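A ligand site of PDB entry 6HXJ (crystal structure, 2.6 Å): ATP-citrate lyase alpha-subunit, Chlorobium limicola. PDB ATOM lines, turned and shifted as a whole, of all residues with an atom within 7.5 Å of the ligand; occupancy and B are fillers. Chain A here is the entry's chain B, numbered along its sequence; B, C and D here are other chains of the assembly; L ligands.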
ATOM      1  N   LEU A 476     -21.401  30.481 -32.438  1.00  0.00           N
ATOM      2  CA  LEU A 476     -21.864  29.295 -31.738  1.00  0.00           C
ATOM      3  C   LEU A 476     -21.922  28.060 -32.647  1.00  0.00           C
ATOM      4  O   LEU A 476     -21.470  26.995 -32.214  1.00  0.00           O
ATOM      5  CB  LEU A 476     -23.198  29.541 -31.020  1.00  0.00           C
ATOM      6  CG  LEU A 476     -23.167  30.563 -29.868  1.00  0.00           C
ATOM      7  CD1 LEU A 476     -24.575  30.918 -29.403  1.00  0.00           C
ATOM      8  CD2 LEU A 476     -22.307  30.069 -28.700  1.00  0.00           C
ATOM      9  N   SER A 477     -22.385  28.215 -33.919  1.00  0.00           N
ATOM     10  CA  SER A 477     -22.406  27.094 -34.865  1.00  0.00           C
ATOM     11  C   SER A 477     -20.977  26.600 -35.171  1.00  0.00           C
ATOM     12  O   SER A 477     -20.687  25.401 -35.062  1.00  0.00           O
ATOM     13  CB  SER A 477     -23.125  27.476 -36.149  1.00  0.00           C
ATOM     14  OG  SER A 477     -24.485  27.753 -35.845  1.00  0.00           O
ATOM     15  N   MET A 479     -18.382  26.972 -33.245  1.00  0.00           N
ATOM     16  CA  MET A 479     -17.849  26.342 -32.023  1.00  0.00           C
ATOM     17  C   MET A 479     -18.327  24.926 -31.807  1.00  0.00           C
ATOM     18  O   MET A 479     -17.535  24.072 -31.411  1.00  0.00           O
ATOM     19  CB  MET A 479     -18.126  27.197 -30.771  1.00  0.00           C
ATOM     20  CG  MET A 479     -17.376  28.505 -30.738  1.00  0.00           C
ATOM     21  SD  MET A 479     -15.589  28.353 -30.608  1.00  0.00           S
ATOM     22  CE  MET A 479     -15.419  27.973 -28.902  1.00  0.00           C
ATOM     23  N   LYS A 480     -19.639  24.688 -32.057  1.00  0.00           N
ATOM     24  CA  LYS A 480     -20.281  23.376 -31.899  1.00  0.00           C
ATOM     25  C   LYS A 480     -19.625  22.353 -32.837  1.00  0.00           C
ATOM     26  O   LYS A 480     -19.213  21.266 -32.398  1.00  0.00           O
ATOM     27  CB  LYS A 480     -21.793  23.484 -32.187  1.00  0.00           C
ATOM     28  CG  LYS A 480     -22.604  22.368 -31.561  1.00  0.00           C
ATOM     29  CD  LYS A 480     -24.076  22.548 -31.857  1.00  0.00           C
ATOM     30  CE  LYS A 480     -24.904  21.441 -31.240  1.00  0.00           C
ATOM     31  NZ  LYS A 480     -26.279  21.438 -31.795  1.00  0.00           N
ATOM     32  N   GLY A 484     -16.534  22.080 -29.754  1.00  0.00           N
ATOM     33  CA  GLY A 484     -17.473  21.421 -28.860  1.00  0.00           C
ATOM     34  C   GLY A 484     -18.097  22.453 -27.938  1.00  0.00           C
ATOM     35  O   GLY A 484     -18.549  23.512 -28.414  1.00  0.00           O
ATOM     36  N   PRO A 485     -18.119  22.221 -26.587  1.00  0.00           N
ATOM     37  CA  PRO A 485     -18.677  23.257 -25.698  1.00  0.00           C
ATOM     38  C   PRO A 485     -17.792  24.508 -25.694  1.00  0.00           C
ATOM     39  O   PRO A 485     -16.558  24.405 -25.868  1.00  0.00           O
ATOM     40  CB  PRO A 485     -18.749  22.556 -24.337  1.00  0.00           C
ATOM     41  CG  PRO A 485     -17.731  21.490 -24.413  1.00  0.00           C
ATOM     42  CD  PRO A 485     -17.629  21.054 -25.823  1.00  0.00           C
ATOM     43  N   VAL A 486     -18.430  25.689 -25.576  1.00  0.00           N
ATOM     44  CA  VAL A 486     -17.713  26.959 -25.563  1.00  0.00           C
ATOM     45  C   VAL A 486     -16.911  27.126 -24.260  1.00  0.00           C
ATOM     46  O   VAL A 486     -17.542  27.093 -23.196  1.00  0.00           O
ATOM     47  CB  VAL A 486     -18.677  28.153 -25.789  1.00  0.00           C
ATOM     48  CG1 VAL A 486     -17.945  29.497 -25.675  1.00  0.00           C
ATOM     49  CG2 VAL A 486     -19.357  28.035 -27.140  1.00  0.00           C
ATOM     50  N   PRO A 487     -15.549  27.270 -24.318  1.00  0.00           N
ATOM     51  CA  PRO A 487     -14.762  27.494 -23.086  1.00  0.00           C
ATOM     52  C   PRO A 487     -15.203  28.815 -22.425  1.00  0.00           C
ATOM     53  O   PRO A 487     -15.366  29.829 -23.129  1.00  0.00           O
ATOM     54  CB  PRO A 487     -13.323  27.624 -23.610  1.00  0.00           C
ATOM     55  CG  PRO A 487     -13.326  26.979 -24.925  1.00  0.00           C
ATOM     56  CD  PRO A 487     -14.661  27.312 -25.512  1.00  0.00           C
ATOM     57  N   GLY A 488     -15.470  28.759 -21.124  1.00  0.00           N
ATOM     58  CA  GLY A 488     -15.930  29.936 -20.379  1.00  0.00           C
ATOM     59  C   GLY A 488     -17.428  30.056 -20.176  1.00  0.00           C
ATOM     60  O   GLY A 488     -17.871  30.980 -19.505  1.00  0.00           O
ATOM     61  N   ILE A 489     -18.203  29.131 -20.768  1.00  0.00           N
ATOM     62  CA  ILE A 489     -19.651  29.059 -20.655  1.00  0.00           C
ATOM     63  C   ILE A 489     -20.025  27.766 -19.938  1.00  0.00           C
ATOM     64  O   ILE A 489     -19.479  26.723 -20.273  1.00  0.00           O
ATOM     65  CB  ILE A 489     -20.313  29.138 -22.062  1.00  0.00           C
ATOM     66  CG1 ILE A 489     -20.152  30.543 -22.720  1.00  0.00           C
ATOM     67  CG2 ILE A 489     -21.791  28.649 -22.058  1.00  0.00           C
ATOM     68  CD1 ILE A 489     -21.110  31.675 -22.253  1.00  0.00           C
ATOM     69  N   GLY A 490     -20.957  27.853 -18.994  1.00  0.00           N
ATOM     70  CA  GLY A 490     -21.469  26.715 -18.236  1.00  0.00           C
ATOM     71  C   GLY A 490     -20.957  26.580 -16.812  1.00  0.00           C
ATOM     72  O   GLY A 490     -19.814  26.953 -16.526  1.00  0.00           O
ATOM     73  N   HIS A 491     -21.806  26.044 -15.906  1.00  0.00           N
ATOM     74  CA  HIS A 491     -21.485  25.784 -14.510  1.00  0.00           C
ATOM     75  C   HIS A 491     -22.394  24.674 -13.971  1.00  0.00           C
ATOM     76  O   HIS A 491     -23.545  24.591 -14.379  1.00  0.00           O
ATOM     77  CB  HIS A 491     -21.609  27.058 -13.658  1.00  0.00           C
ATOM     78  CG  HIS A 491     -20.754  27.012 -12.425  1.00  0.00           C
ATOM     79  ND1 HIS A 491     -21.188  26.396 -11.247  1.00  0.00           N
ATOM     80  CD2 HIS A 491     -19.474  27.423 -12.247  1.00  0.00           C
ATOM     81  CE1 HIS A 491     -20.180  26.477 -10.396  1.00  0.00           C
ATOM     82  NE2 HIS A 491     -19.119  27.072 -10.945  1.00  0.00           N
ATOM     83  N   VAL A 527     -23.157  36.575 -25.750  1.00  0.00           N
ATOM     84  CA  VAL A 527     -23.351  35.135 -26.018  1.00  0.00           C
ATOM     85  C   VAL A 527     -24.017  34.458 -24.787  1.00  0.00           C
ATOM     86  O   VAL A 527     -24.861  33.588 -24.981  1.00  0.00           O
ATOM     87  CB  VAL A 527     -22.137  34.333 -26.596  1.00  0.00           C
ATOM     88  CG1 VAL A 527     -20.912  35.190 -26.851  1.00  0.00           C
ATOM     89  CG2 VAL A 527     -21.809  33.067 -25.813  1.00  0.00           C
ATOM     90  N   THR A 531     -26.918  31.670 -24.864  1.00  0.00           N
ATOM     91  CA  THR A 531     -26.705  30.331 -24.281  1.00  0.00           C
ATOM     92  C   THR A 531     -27.672  30.051 -23.107  1.00  0.00           C
ATOM     93  O   THR A 531     -28.240  28.951 -23.056  1.00  0.00           O
ATOM     94  CB  THR A 531     -25.226  30.096 -23.892  1.00  0.00           C
ATOM     95  OG1 THR A 531     -24.783  31.082 -22.958  1.00  0.00           O
ATOM     96  CG2 THR A 531     -24.284  30.039 -25.104  1.00  0.00           C
ATOM     97  N   LYS A 534     -30.992  28.829 -24.050  1.00  0.00           N
ATOM     98  CA  LYS A 534     -30.966  27.391 -24.373  1.00  0.00           C
ATOM     99  C   LYS A 534     -31.036  26.558 -23.072  1.00  0.00           C
ATOM    100  O   LYS A 534     -31.961  25.754 -22.923  1.00  0.00           O
ATOM    101  CB  LYS A 534     -29.692  27.020 -25.176  1.00  0.00           C
ATOM    102  CG  LYS A 534     -29.552  27.749 -26.510  1.00  0.00           C
ATOM    103  CD  LYS A 534     -28.271  27.374 -27.223  1.00  0.00           C
ATOM    104  CE  LYS A 534     -28.180  28.028 -28.570  1.00  0.00           C
ATOM    105  NZ  LYS A 534     -27.128  27.396 -29.403  1.00  0.00           N
ATOM    106  N   LYS A 535     -30.069  26.755 -22.143  1.00  0.00           N
ATOM    107  CA  LYS A 535     -29.988  26.099 -20.818  1.00  0.00           C
ATOM    108  C   LYS A 535     -29.596  27.148 -19.794  1.00  0.00           C
ATOM    109  O   LYS A 535     -28.550  27.789 -19.941  1.00  0.00           O
ATOM    110  CB  LYS A 535     -28.921  24.981 -20.784  1.00  0.00           C
ATOM    111  CG  LYS A 535     -29.253  23.641 -21.430  1.00  0.00           C
ATOM    112  CD  LYS A 535     -28.292  22.560 -20.896  1.00  0.00           C
ATOM    113  CE  LYS A 535     -28.790  21.841 -19.666  1.00  0.00           C
ATOM    114  NZ  LYS A 535     -27.834  20.806 -19.215  1.00  0.00           N
ATOM    115  N   ASN A 537     -28.096  27.005 -17.018  1.00  0.00           N
ATOM    116  CA  ASN A 537     -26.766  26.846 -16.400  1.00  0.00           C
ATOM    117  C   ASN A 537     -25.628  27.272 -17.354  1.00  0.00           C
ATOM    118  O   ASN A 537     -24.465  27.282 -16.945  1.00  0.00           O
ATOM    119  CB  ASN A 537     -26.556  25.418 -15.876  1.00  0.00           C
ATOM    120  CG  ASN A 537     -26.277  24.388 -16.933  1.00  0.00           C
ATOM    121  OD1 ASN A 537     -27.005  24.222 -17.913  1.00  0.00           O
ATOM    122  ND2 ASN A 537     -25.200  23.648 -16.766  1.00  0.00           N
ATOM    123  N   LEU A 538     -25.951  27.626 -18.601  1.00  0.00           N
ATOM    124  CA  LEU A 538     -24.936  28.044 -19.565  1.00  0.00           C
ATOM    125  C   LEU A 538     -24.545  29.511 -19.393  1.00  0.00           C
ATOM    126  O   LEU A 538     -24.494  30.286 -20.354  1.00  0.00           O
ATOM    127  CB  LEU A 538     -25.350  27.711 -21.007  1.00  0.00           C
ATOM    128  CG  LEU A 538     -25.500  26.266 -21.332  1.00  0.00           C
ATOM    129  CD1 LEU A 538     -25.939  26.103 -22.754  1.00  0.00           C
ATOM    130  CD2 LEU A 538     -24.238  25.481 -21.002  1.00  0.00           C
ATOM    131  N   ILE A 539     -24.238  29.862 -18.139  1.00  0.00           N
ATOM    132  CA  ILE A 539     -23.810  31.180 -17.687  1.00  0.00           C
ATOM    133  C   ILE A 539     -22.361  31.418 -18.098  1.00  0.00           C
ATOM    134  O   ILE A 539     -21.625  30.455 -18.245  1.00  0.00           O
ATOM    135  CB  ILE A 539     -24.023  31.317 -16.128  1.00  0.00           C
ATOM    136  CG1 ILE A 539     -23.349  30.204 -15.302  1.00  0.00           C
ATOM    137  CG2 ILE A 539     -25.484  31.386 -15.776  1.00  0.00           C
ATOM    138  CD1 ILE A 539     -22.001  30.563 -14.752  1.00  0.00           C
ATOM    139  N   ASN A 541     -18.950  31.841 -16.990  1.00  0.00           N
ATOM    140  CA  ASN A 541     -18.317  31.483 -15.701  1.00  0.00           C
ATOM    141  C   ASN A 541     -17.039  32.330 -15.394  1.00  0.00           C
ATOM    142  O   ASN A 541     -16.670  33.181 -16.206  1.00  0.00           O
ATOM    143  CB  ASN A 541     -18.051  29.951 -15.617  1.00  0.00           C
ATOM    144  CG  ASN A 541     -17.161  29.448 -16.714  1.00  0.00           C
ATOM    145  OD1 ASN A 541     -16.163  30.062 -17.086  1.00  0.00           O
ATOM    146  ND2 ASN A 541     -17.514  28.306 -17.267  1.00  0.00           N
ATOM    147  N   ARG B 585     -18.722  12.708 -17.035  1.00  0.00           N
ATOM    148  CA  ARG B 585     -18.778  14.151 -16.808  1.00  0.00           C
ATOM    149  C   ARG B 585     -17.888  14.462 -15.598  1.00  0.00           C
ATOM    150  O   ARG B 585     -17.572  13.562 -14.803  1.00  0.00           O
ATOM    151  CB  ARG B 585     -20.222  14.548 -16.481  1.00  0.00           C
ATOM    152  CG  ARG B 585     -21.193  14.437 -17.666  1.00  0.00           C
ATOM    153  CD  ARG B 585     -22.650  14.243 -17.224  1.00  0.00           C
ATOM    154  NE  ARG B 585     -23.288  15.465 -16.720  1.00  0.00           N
ATOM    155  CZ  ARG B 585     -23.680  15.652 -15.455  1.00  0.00           C
ATOM    156  NH1 ARG B 585     -23.475  14.717 -14.534  1.00  0.00           N
ATOM    157  NH2 ARG B 585     -24.275  16.787 -15.108  1.00  0.00           N
ATOM    158  N   VAL C  17     -31.752   8.535 -25.852  1.00  0.00           N
ATOM    159  CA  VAL C  17     -32.235   9.108 -24.594  1.00  0.00           C
ATOM    160  C   VAL C  17     -33.743   8.906 -24.399  1.00  0.00           C
ATOM    161  O   VAL C  17     -34.155   8.555 -23.292  1.00  0.00           O
ATOM    162  CB  VAL C  17     -31.769  10.578 -24.382  1.00  0.00           C
ATOM    163  CG1 VAL C  17     -32.425  11.542 -25.370  1.00  0.00           C
ATOM    164  CG2 VAL C  17     -32.001  11.028 -22.943  1.00  0.00           C
ATOM    165  N   ARG D 246     -38.641  23.681 -34.794  1.00  0.00           N
ATOM    166  CA  ARG D 246     -37.486  24.255 -34.095  1.00  0.00           C
ATOM    167  C   ARG D 246     -37.250  23.444 -32.815  1.00  0.00           C
ATOM    168  O   ARG D 246     -36.104  23.321 -32.350  1.00  0.00           O
ATOM    169  CB  ARG D 246     -37.716  25.744 -33.778  1.00  0.00           C
ATOM    170  CG  ARG D 246     -37.323  26.661 -34.933  1.00  0.00           C
ATOM    171  CD  ARG D 246     -37.949  28.038 -34.823  1.00  0.00           C
ATOM    172  NE  ARG D 246     -37.368  28.969 -35.791  1.00  0.00           N
ATOM    173  CZ  ARG D 246     -37.877  30.170 -36.098  1.00  0.00           C
ATOM    174  NH1 ARG D 246     -38.993  30.584 -35.505  1.00  0.00           N
ATOM    175  NH2 ARG D 246     -37.279  30.947 -36.977  1.00  0.00           N
HETATM  176  N1  LIG L   1     -21.208  25.956 -24.295  1.00  0.00           N
HETATM  177  C1  LIG L   1     -22.058  26.352 -25.257  1.00  0.00           C
HETATM  178  N2  LIG L   1     -23.189  25.777 -25.656  1.00  0.00           N
HETATM  179  C2  LIG L   1     -23.437  24.657 -24.963  1.00  0.00           C
HETATM  180  C3  LIG L   1     -22.652  24.117 -23.958  1.00  0.00           C
HETATM  181  C4  LIG L   1     -21.485  24.830 -23.604  1.00  0.00           C
HETATM  182  N3  LIG L   1     -20.722  24.534 -22.551  1.00  0.00           N
HETATM  183  N4  LIG L   1     -23.236  22.953 -23.460  1.00  0.00           N
HETATM  184  C5  LIG L   1     -24.334  22.832 -24.164  1.00  0.00           C
HETATM  185  N5  LIG L   1     -24.522  23.818 -25.089  1.00  0.00           N
HETATM  186  C6  LIG L   1     -25.648  23.957 -26.015  1.00  0.00           C
HETATM  187  C7  LIG L   1     -25.840  22.772 -26.967  1.00  0.00           C
HETATM  188  O1  LIG L   1     -24.986  22.848 -28.108  1.00  0.00           O
HETATM  189  C8  LIG L   1     -27.326  22.891 -27.278  1.00  0.00           C
HETATM  190  O2  LIG L   1     -27.554  23.937 -28.248  1.00  0.00           O
HETATM  191  P1  LIG L   1     -28.094  23.775 -29.770  1.00  0.00           P
HETATM  192  O3  LIG L   1     -28.310  22.329 -30.116  1.00  0.00           O
HETATM  193  O4  LIG L   1     -29.390  24.612 -29.803  1.00  0.00           O
HETATM  194  O5  LIG L   1     -27.026  24.437 -30.659  1.00  0.00           O
HETATM  195  C9  LIG L   1     -27.923  23.391 -25.956  1.00  0.00           C
HETATM  196  O6  LIG L   1     -26.846  24.064 -25.275  1.00  0.00           O
HETATM  197  C10 LIG L   1     -28.557  22.375 -25.028  1.00  0.00           C
HETATM  198  O7  LIG L   1     -27.770  21.164 -24.945  1.00  0.00           O
HETATM  199  P2  LIG L   1     -28.292  19.824 -25.746  1.00  0.00           P
HETATM  200  O8  LIG L   1     -29.344  20.060 -26.775  1.00  0.00           O
HETATM  201  O9  LIG L   1     -27.071  19.077 -26.276  1.00  0.00           O
HETATM  202  O10 LIG L   1     -28.886  18.940 -24.574  1.00  0.00           O
HETATM  203  P3  LIG L   1     -28.153  18.444 -23.259  1.00  0.00           P
HETATM  204  O11 LIG L   1     -28.694  19.197 -22.101  1.00  0.00           O
HETATM  205  O12 LIG L   1     -28.342  16.916 -23.189  1.00  0.00           O
HETATM  206  O13 LIG L   1     -26.543  18.750 -23.528  1.00  0.00           O
HETATM  207  C11 LIG L   1     -24.306  18.790 -22.539  1.00  0.00           C
HETATM  208  C12 LIG L   1     -25.518  17.941 -22.923  1.00  0.00           C
HETATM  209  C13 LIG L   1     -23.538  19.141 -23.815  1.00  0.00           C
HETATM  210  C14 LIG L   1     -23.393  17.943 -21.642  1.00  0.00           C
HETATM  211  C15 LIG L   1     -24.622  20.109 -21.774  1.00  0.00           C
HETATM  212  O14 LIG L   1     -25.637  20.025 -20.789  1.00  0.00           O
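The side-chain amino group (NZ) of Lys 534 is in salt-bridge range of an oxygen (O5) of the ligand, at 3.2 Å. The side-chain amino group (NZ) of Lys 480 lies within salt-bridge range of an oxygen (O3) of the ligand (2.8 Å). The side-chain amino group of Lys 535 lies within salt-bridge range of an oxygen (O11) of the ligand, 3.4 Å away. A nitrogen (N3) of the ligand is in hydrogen-bond range of the backbone carbonyl oxygen (O) of Ile 489 (3.4 Å). A nitrogen (N1) of the ligand is in hydrogen-bond range of the backbone NH (N) of Val 486, 3.1 Å away.
O of Leu 538 is in hydrogen-bond range of OG1 of Thr 531, 2.7 Å away.
Pro 485 touches the ligand. Leu 538 touches the ligand (CD1 to O6, 3.4 Å). Hydrophobic or aromatic side chains that line the ligand: Pro 485, Val 486, Ile 489 and Leu 538. Within 4 Å of the ligand: Lys 480, Pro 485, Val 486, Ile 489, Lys 534, Lys 535 and Leu 538.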
